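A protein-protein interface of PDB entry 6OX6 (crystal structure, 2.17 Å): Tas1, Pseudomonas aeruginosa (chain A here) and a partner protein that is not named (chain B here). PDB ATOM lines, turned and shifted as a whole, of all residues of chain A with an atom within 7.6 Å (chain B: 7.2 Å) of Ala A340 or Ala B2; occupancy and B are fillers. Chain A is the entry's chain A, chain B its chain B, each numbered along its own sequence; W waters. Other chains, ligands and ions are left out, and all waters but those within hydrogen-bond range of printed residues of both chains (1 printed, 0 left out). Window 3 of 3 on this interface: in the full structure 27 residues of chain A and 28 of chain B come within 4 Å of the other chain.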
ATOM      1  N   VAL A 335       7.291  -2.256   8.648  1.00  0.00           N
ATOM      2  CA  VAL A 335       6.116  -1.716   7.979  1.00  0.00           C
ATOM      3  C   VAL A 335       5.957  -2.484   6.673  1.00  0.00           C
ATOM      4  O   VAL A 335       6.822  -2.425   5.788  1.00  0.00           O
ATOM      5  CB  VAL A 335       6.225  -0.211   7.735  1.00  0.00           C
ATOM      6  CG1 VAL A 335       5.059   0.222   6.902  1.00  0.00           C
ATOM      7  CG2 VAL A 335       6.259   0.555   9.072  1.00  0.00           C
ATOM      8  N   ILE A 336       4.866  -3.231   6.560  1.00  0.00           N
ATOM      9  CA  ILE A 336       4.621  -4.084   5.407  1.00  0.00           C
ATOM     10  C   ILE A 336       3.674  -3.355   4.472  1.00  0.00           C
ATOM     11  O   ILE A 336       2.553  -3.004   4.859  1.00  0.00           O
ATOM     12  CB  ILE A 336       4.029  -5.431   5.846  1.00  0.00           C
ATOM     13  CG1 ILE A 336       5.037  -6.162   6.725  1.00  0.00           C
ATOM     14  CG2 ILE A 336       3.624  -6.253   4.650  1.00  0.00           C
ATOM     15  CD1 ILE A 336       4.385  -7.004   7.816  1.00  0.00           C
ATOM     16  N   ASP A 337       4.087  -3.131   3.239  1.00  0.00           N
ATOM     17  CA  ASP A 337       3.093  -2.688   2.275  1.00  0.00           C
ATOM     18  C   ASP A 337       2.829  -3.802   1.272  1.00  0.00           C
ATOM     19  O   ASP A 337       3.664  -4.697   1.040  1.00  0.00           O
ATOM     20  CB  ASP A 337       3.504  -1.401   1.555  1.00  0.00           C
ATOM     21  CG  ASP A 337       4.596  -1.625   0.531  1.00  0.00           C
ATOM     22  OD1 ASP A 337       5.694  -2.106   0.882  1.00  0.00           O
ATOM     23  OD2 ASP A 337       4.338  -1.330  -0.636  1.00  0.00           O
ATOM     24  N   GLY A 338       1.635  -3.738   0.687  1.00  0.00           N
ATOM     25  CA  GLY A 338       1.199  -4.772  -0.224  1.00  0.00           C
ATOM     26  C   GLY A 338       1.982  -4.857  -1.514  1.00  0.00           C
ATOM     27  O   GLY A 338       1.797  -5.833  -2.244  1.00  0.00           O
ATOM     28  N   ASN A 339       2.853  -3.887  -1.811  1.00  0.00           N
ATOM     29  CA  ASN A 339       3.562  -3.888  -3.090  1.00  0.00           C
ATOM     30  C   ASN A 339       4.882  -4.645  -3.051  1.00  0.00           C
ATOM     31  O   ASN A 339       5.447  -4.911  -4.115  1.00  0.00           O
ATOM     32  CB  ASN A 339       3.818  -2.458  -3.571  1.00  0.00           C
ATOM     33  CG  ASN A 339       2.518  -1.667  -3.772  1.00  0.00           C
ATOM     34  OD1 ASN A 339       1.521  -2.188  -4.312  1.00  0.00           O
ATOM     35  ND2 ASN A 339       2.509  -0.416  -3.283  1.00  0.00           N
ATOM     36  N   ALA A 340       5.369  -5.017  -1.868  1.00  0.00           N
ATOM     37  CA  ALA A 340       6.609  -5.781  -1.732  1.00  0.00           C
ATOM     38  C   ALA A 340       6.376  -7.219  -1.289  1.00  0.00           C
ATOM     39  O   ALA A 340       6.926  -8.157  -1.880  1.00  0.00           O
ATOM     40  CB  ALA A 340       7.543  -5.072  -0.736  1.00  0.00           C
ATOM     41  N   ASP A 341       5.571  -7.419  -0.257  1.00  0.00           N
ATOM     42  CA  ASP A 341       5.189  -8.753   0.183  1.00  0.00           C
ATOM     43  C   ASP A 341       4.630  -9.571  -0.994  1.00  0.00           C
ATOM     44  O   ASP A 341       3.661  -9.132  -1.635  1.00  0.00           O
ATOM     45  CB  ASP A 341       4.152  -8.602   1.290  1.00  0.00           C
ATOM     46  CG  ASP A 341       3.569  -9.930   1.752  1.00  0.00           C
ATOM     47  OD1 ASP A 341       4.183 -11.001   1.539  1.00  0.00           O
ATOM     48  OD2 ASP A 341       2.489  -9.893   2.365  1.00  0.00           O
ATOM     49  N   PRO A 342       5.185 -10.758  -1.292  1.00  0.00           N
ATOM     50  CA  PRO A 342       4.633 -11.563  -2.397  1.00  0.00           C
ATOM     51  C   PRO A 342       3.162 -11.874  -2.222  1.00  0.00           C
ATOM     52  O   PRO A 342       2.452 -12.089  -3.215  1.00  0.00           O
ATOM     53  CB  PRO A 342       5.466 -12.854  -2.353  1.00  0.00           C
ATOM     54  CG  PRO A 342       6.675 -12.522  -1.540  1.00  0.00           C
ATOM     55  CD  PRO A 342       6.227 -11.503  -0.548  1.00  0.00           C
ATOM     56  N   LEU A 343       2.682 -11.913  -0.986  1.00  0.00           N
ATOM     57  CA  LEU A 343       1.283 -12.189  -0.711  1.00  0.00           C
ATOM     58  C   LEU A 343       0.430 -10.927  -0.573  1.00  0.00           C
ATOM     59  O   LEU A 343      -0.765 -11.048  -0.327  1.00  0.00           O
ATOM     60  CB  LEU A 343       1.160 -13.025   0.564  1.00  0.00           C
ATOM     61  CG  LEU A 343       1.984 -14.331   0.625  1.00  0.00           C
ATOM     62  CD1 LEU A 343       1.544 -15.157   1.873  1.00  0.00           C
ATOM     63  CD2 LEU A 343       1.890 -15.155  -0.611  1.00  0.00           C
ATOM     64  N   GLY A 344       1.000  -9.736  -0.716  1.00  0.00           N
ATOM     65  CA  GLY A 344       0.194  -8.520  -0.772  1.00  0.00           C
ATOM     66  C   GLY A 344      -0.427  -8.083   0.536  1.00  0.00           C
ATOM     67  O   GLY A 344      -1.297  -7.200   0.535  1.00  0.00           O
ATOM     68  N   TYR A 345       0.023  -8.633   1.655  1.00  0.00           N
ATOM     69  CA  TYR A 345      -0.502  -8.231   2.945  1.00  0.00           C
ATOM     70  C   TYR A 345       0.026  -6.836   3.309  1.00  0.00           C
ATOM     71  O   TYR A 345       1.041  -6.375   2.777  1.00  0.00           O
ATOM     72  CB  TYR A 345      -0.113  -9.282   4.001  1.00  0.00           C
ATOM     73  CG  TYR A 345      -0.624  -9.021   5.414  1.00  0.00           C
ATOM     74  CD1 TYR A 345       0.265  -8.826   6.460  1.00  0.00           C
ATOM     75  CD2 TYR A 345      -1.986  -8.957   5.684  1.00  0.00           C
ATOM     76  CE1 TYR A 345      -0.190  -8.577   7.761  1.00  0.00           C
ATOM     77  CE2 TYR A 345      -2.457  -8.721   6.969  1.00  0.00           C
ATOM     78  CZ  TYR A 345      -1.546  -8.541   7.999  1.00  0.00           C
ATOM     79  OH  TYR A 345      -1.973  -8.293   9.273  1.00  0.00           O
ATOM     80  N   ARG A 427      -2.487 -11.463  -3.487  1.00  0.00           N
ATOM     81  CA  ARG A 427      -2.344 -10.033  -3.729  1.00  0.00           C
ATOM     82  C   ARG A 427      -3.631  -9.459  -4.291  1.00  0.00           C
ATOM     83  O   ARG A 427      -4.072  -8.379  -3.877  1.00  0.00           O
ATOM     84  CB  ARG A 427      -1.200  -9.759  -4.709  1.00  0.00           C
ATOM     85  CG  ARG A 427       0.179 -10.091  -4.165  1.00  0.00           C
ATOM     86  CD  ARG A 427       1.286  -9.494  -5.060  1.00  0.00           C
ATOM     87  NE  ARG A 427       1.235 -10.030  -6.414  1.00  0.00           N
ATOM     88  CZ  ARG A 427       1.776 -11.197  -6.775  1.00  0.00           C
ATOM     89  NH1 ARG A 427       2.430 -11.943  -5.881  1.00  0.00           N
ATOM     90  NH2 ARG A 427       1.690 -11.606  -8.036  1.00  0.00           N
ATOM     91  N   ALA B   2      11.694  -8.685  -0.771  1.00  0.00           N
ATOM     92  CA  ALA B   2      11.175 -10.057  -0.936  1.00  0.00           C
ATOM     93  C   ALA B   2      11.964 -10.928  -1.941  1.00  0.00           C
ATOM     94  O   ALA B   2      12.556 -10.420  -2.904  1.00  0.00           O
ATOM     95  CB  ALA B   2       9.718 -10.006  -1.359  1.00  0.00           C
ATOM     96  N   ILE B   3      11.929 -12.244  -1.709  1.00  0.00           N
ATOM     97  CA  ILE B   3      12.510 -13.245  -2.600  1.00  0.00           C
ATOM     98  C   ILE B   3      11.401 -14.266  -2.863  1.00  0.00           C
ATOM     99  O   ILE B   3      11.149 -15.145  -2.030  1.00  0.00           O
ATOM    100  CB  ILE B   3      13.755 -13.915  -1.994  1.00  0.00           C
ATOM    101  CG1 ILE B   3      14.746 -12.849  -1.485  1.00  0.00           C
ATOM    102  CG2 ILE B   3      14.451 -14.807  -3.017  1.00  0.00           C
ATOM    103  CD1 ILE B   3      14.703 -12.577   0.012  1.00  0.00           C
ATOM    104  N   GLU B   4      10.729 -14.148  -4.010  1.00  0.00           N
ATOM    105  CA  GLU B   4       9.565 -14.974  -4.309  1.00  0.00           C
ATOM    106  C   GLU B   4       9.980 -16.417  -4.572  1.00  0.00           C
ATOM    107  O   GLU B   4      11.060 -16.678  -5.103  1.00  0.00           O
ATOM    108  CB  GLU B   4       8.828 -14.424  -5.538  1.00  0.00           C
ATOM    109  CG  GLU B   4       8.171 -13.035  -5.353  1.00  0.00           C
ATOM    110  CD  GLU B   4       9.121 -11.835  -5.593  1.00  0.00           C
ATOM    111  OE1 GLU B   4      10.351 -12.044  -5.772  1.00  0.00           O
ATOM    112  OE2 GLU B   4       8.631 -10.675  -5.616  1.00  0.00           O
ATOM    113  N   ASP B  57       9.049 -16.143   6.463  1.00  0.00           N
ATOM    114  CA  ASP B  57       9.029 -14.703   6.740  1.00  0.00           C
ATOM    115  C   ASP B  57      10.166 -14.000   6.011  1.00  0.00           C
ATOM    116  O   ASP B  57       9.990 -12.893   5.478  1.00  0.00           O
ATOM    117  CB  ASP B  57       9.106 -14.428   8.244  1.00  0.00           C
ATOM    118  CG  ASP B  57       7.750 -14.552   8.937  1.00  0.00           C
ATOM    119  OD1 ASP B  57       6.766 -14.883   8.261  1.00  0.00           O
ATOM    120  OD2 ASP B  57       7.655 -14.303  10.163  1.00  0.00           O
ATOM    121  N   ALA B  58      11.342 -14.624   5.996  1.00  0.00           N
ATOM    122  CA  ALA B  58      12.499 -14.051   5.316  1.00  0.00           C
ATOM    123  C   ALA B  58      12.241 -13.909   3.831  1.00  0.00           C
ATOM    124  O   ALA B  58      12.633 -12.909   3.220  1.00  0.00           O
ATOM    125  CB  ALA B  58      13.732 -14.914   5.573  1.00  0.00           C
ATOM    126  N   LEU B  59      11.534 -14.871   3.234  1.00  0.00           N
ATOM    127  CA  LEU B  59      11.196 -14.736   1.818  1.00  0.00           C
ATOM    128  C   LEU B  59      10.263 -13.570   1.595  1.00  0.00           C
ATOM    129  O   LEU B  59      10.396 -12.846   0.599  1.00  0.00           O
ATOM    130  CB  LEU B  59      10.550 -16.001   1.277  1.00  0.00           C
ATOM    131  CG  LEU B  59      11.399 -17.254   1.393  1.00  0.00           C
ATOM    132  CD1 LEU B  59      10.737 -18.424   0.647  1.00  0.00           C
ATOM    133  CD2 LEU B  59      12.774 -16.983   0.836  1.00  0.00           C
ATOM    134  N   ARG B  60       9.306 -13.366   2.506  1.00  0.00           N
ATOM    135  CA  ARG B  60       8.304 -12.356   2.220  1.00  0.00           C
ATOM    136  C   ARG B  60       8.855 -10.970   2.457  1.00  0.00           C
ATOM    137  O   ARG B  60       8.528 -10.042   1.713  1.00  0.00           O
ATOM    138  CB  ARG B  60       7.039 -12.590   3.056  1.00  0.00           C
ATOM    139  CG  ARG B  60       6.269 -13.846   2.637  1.00  0.00           C
ATOM    140  CD  ARG B  60       5.097 -14.091   3.573  1.00  0.00           C
ATOM    141  NE  ARG B  60       4.135 -12.983   3.582  1.00  0.00           N
ATOM    142  CZ  ARG B  60       3.096 -12.936   4.408  1.00  0.00           C
ATOM    143  NH1 ARG B  60       2.917 -13.914   5.316  1.00  0.00           N
ATOM    144  NH2 ARG B  60       2.261 -11.917   4.353  1.00  0.00           N
ATOM    145  N   PHE B  61       9.687 -10.810   3.480  1.00  0.00           N
ATOM    146  CA  PHE B  61      10.023  -9.486   3.974  1.00  0.00           C
ATOM    147  C   PHE B  61      11.511  -9.174   3.928  1.00  0.00           C
ATOM    148  O   PHE B  61      11.883  -8.041   4.230  1.00  0.00           O
ATOM    149  CB  PHE B  61       9.503  -9.313   5.408  1.00  0.00           C
ATOM    150  CG  PHE B  61       8.050  -9.725   5.586  1.00  0.00           C
ATOM    151  CD1 PHE B  61       7.043  -9.112   4.840  1.00  0.00           C
ATOM    152  CD2 PHE B  61       7.695 -10.683   6.526  1.00  0.00           C
ATOM    153  CE1 PHE B  61       5.705  -9.477   5.010  1.00  0.00           C
ATOM    154  CE2 PHE B  61       6.347 -11.062   6.713  1.00  0.00           C
ATOM    155  CZ  PHE B  61       5.358 -10.462   5.944  1.00  0.00           C
ATOM    156  N   GLY B  62      12.366 -10.153   3.614  1.00  0.00           N
ATOM    157  CA  GLY B  62      13.796  -9.946   3.566  1.00  0.00           C
ATOM    158  C   GLY B  62      14.248  -9.483   2.189  1.00  0.00           C
ATOM    159  O   GLY B  62      13.450  -9.170   1.303  1.00  0.00           O
ATOM    160  N   ARG B  63      15.555  -9.443   2.013  1.00  0.00           N
ATOM    161  CA  ARG B  63      16.134  -8.967   0.767  1.00  0.00           C
ATOM    162  C   ARG B  63      17.257  -9.904   0.356  1.00  0.00           C
ATOM    163  O   ARG B  63      17.884 -10.568   1.193  1.00  0.00           O
ATOM    164  CB  ARG B  63      16.656  -7.527   0.893  1.00  0.00           C
ATOM    165  CG  ARG B  63      17.793  -7.370   1.898  1.00  0.00           C
ATOM    166  CD  ARG B  63      18.004  -5.913   2.304  1.00  0.00           C
ATOM    167  NE  ARG B  63      16.869  -5.367   3.042  1.00  0.00           N
ATOM    168  CZ  ARG B  63      15.987  -4.521   2.525  1.00  0.00           C
ATOM    169  NH1 ARG B  63      16.111  -4.130   1.264  1.00  0.00           N
ATOM    170  NH2 ARG B  63      14.979  -4.072   3.266  1.00  0.00           N
ATOM    171  N   GLU B  64      17.486  -9.971  -0.946  1.00  0.00           N
ATOM    172  CA  GLU B  64      18.534 -10.824  -1.467  1.00  0.00           C
ATOM    173  C   GLU B  64      19.893 -10.152  -1.246  1.00  0.00           C
ATOM    174  O   GLU B  64      20.023  -8.934  -1.370  1.00  0.00           O
ATOM    175  CB  GLU B  64      18.272 -11.113  -2.955  1.00  0.00           C
ATOM    176  CG  GLU B  64      19.268 -12.055  -3.576  1.00  0.00           C
ATOM    177  CD  GLU B  64      18.820 -12.671  -4.897  1.00  0.00           C
ATOM    178  OE1 GLU B  64      17.672 -12.426  -5.344  1.00  0.00           O
ATOM    179  OE2 GLU B  64      19.630 -13.445  -5.463  1.00  0.00           O
HETATM  180  O   HOH W   1       7.219  -8.851  -4.403  1.00  0.00           O
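NH2 of Arg B60 lies within salt-bridge range of OD2 of Asp A341 (2.8 Å).
N of Gly A338 sits close to O of Tyr A345 (3.4 Å).
The backbone NH (N) of Leu A343 lies close to the side-chain carboxylate (OD1) of Asp A341 (3.1 Å).
OD2 of Asp A341 sits at hydrogen-bond distance from N of Gly A344.
N of Tyr A345 is in hydrogen-bond range of OD2 of Asp A341, at 2.9 Å.
O of Pro A342 is in hydrogen-bond range of NH1 of Arg A427 (2.7 Å).
The backbone carbonyl oxygen (O) of Gly B62 sits at hydrogen-bond distance from the backbone NH (N) of Ala B2, at 2.8 Å.
Among the printed residues, merely in contact across the chains: Ala A340 with Ala B2, Pro A342 with Arg B60, Tyr A345 with Arg B60, Leu A343 with Arg B60, Ile A336 with Phe B61, Pro A342 with Ala B2 and Asp A341 with Phe B61.
Ala A340 touches one residue of chain B.
Printed residues of chain A within 4 Å of Ala B2: Ala A340 and Pro A342.
Printed residues of chain A within 4 Å of Arg B60: Asp A341 (2.8 Å), Pro A342 (3.5 Å), Leu A343 (3.7 Å) and Tyr A345 (3.6 Å).
Printed residues of chain B within 4 Å of Ile A336: Phe B61 (3.8 Å).
Of the printed residues of chain B, Asp A341 touches Arg B60 and Phe B61.
Printed residues of chain B within 4 Å of Leu A343: Arg B60 (3.7 Å).
The nearest residue of chain B that does not touch Ala A340 is Arg B60 (4.4 Å).
The nearest residue of chain A that does not touch Ala B2 is Asp A341 (4.9 Å).
The nearest printed residue of chain B that does not touch Leu A343 is Glu B4 (7.1 Å).
Of the 12 printed residues of chain A, 6 touch a printed residue of chain B.
Hydrophobic or aromatic side chains of chain B within 4 Å of the printed part of chain A: Ala B2 and Phe B61.
Water W1 lies within hydrogen-bond range of OE2 of Glu B4 and O of Ala A340.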
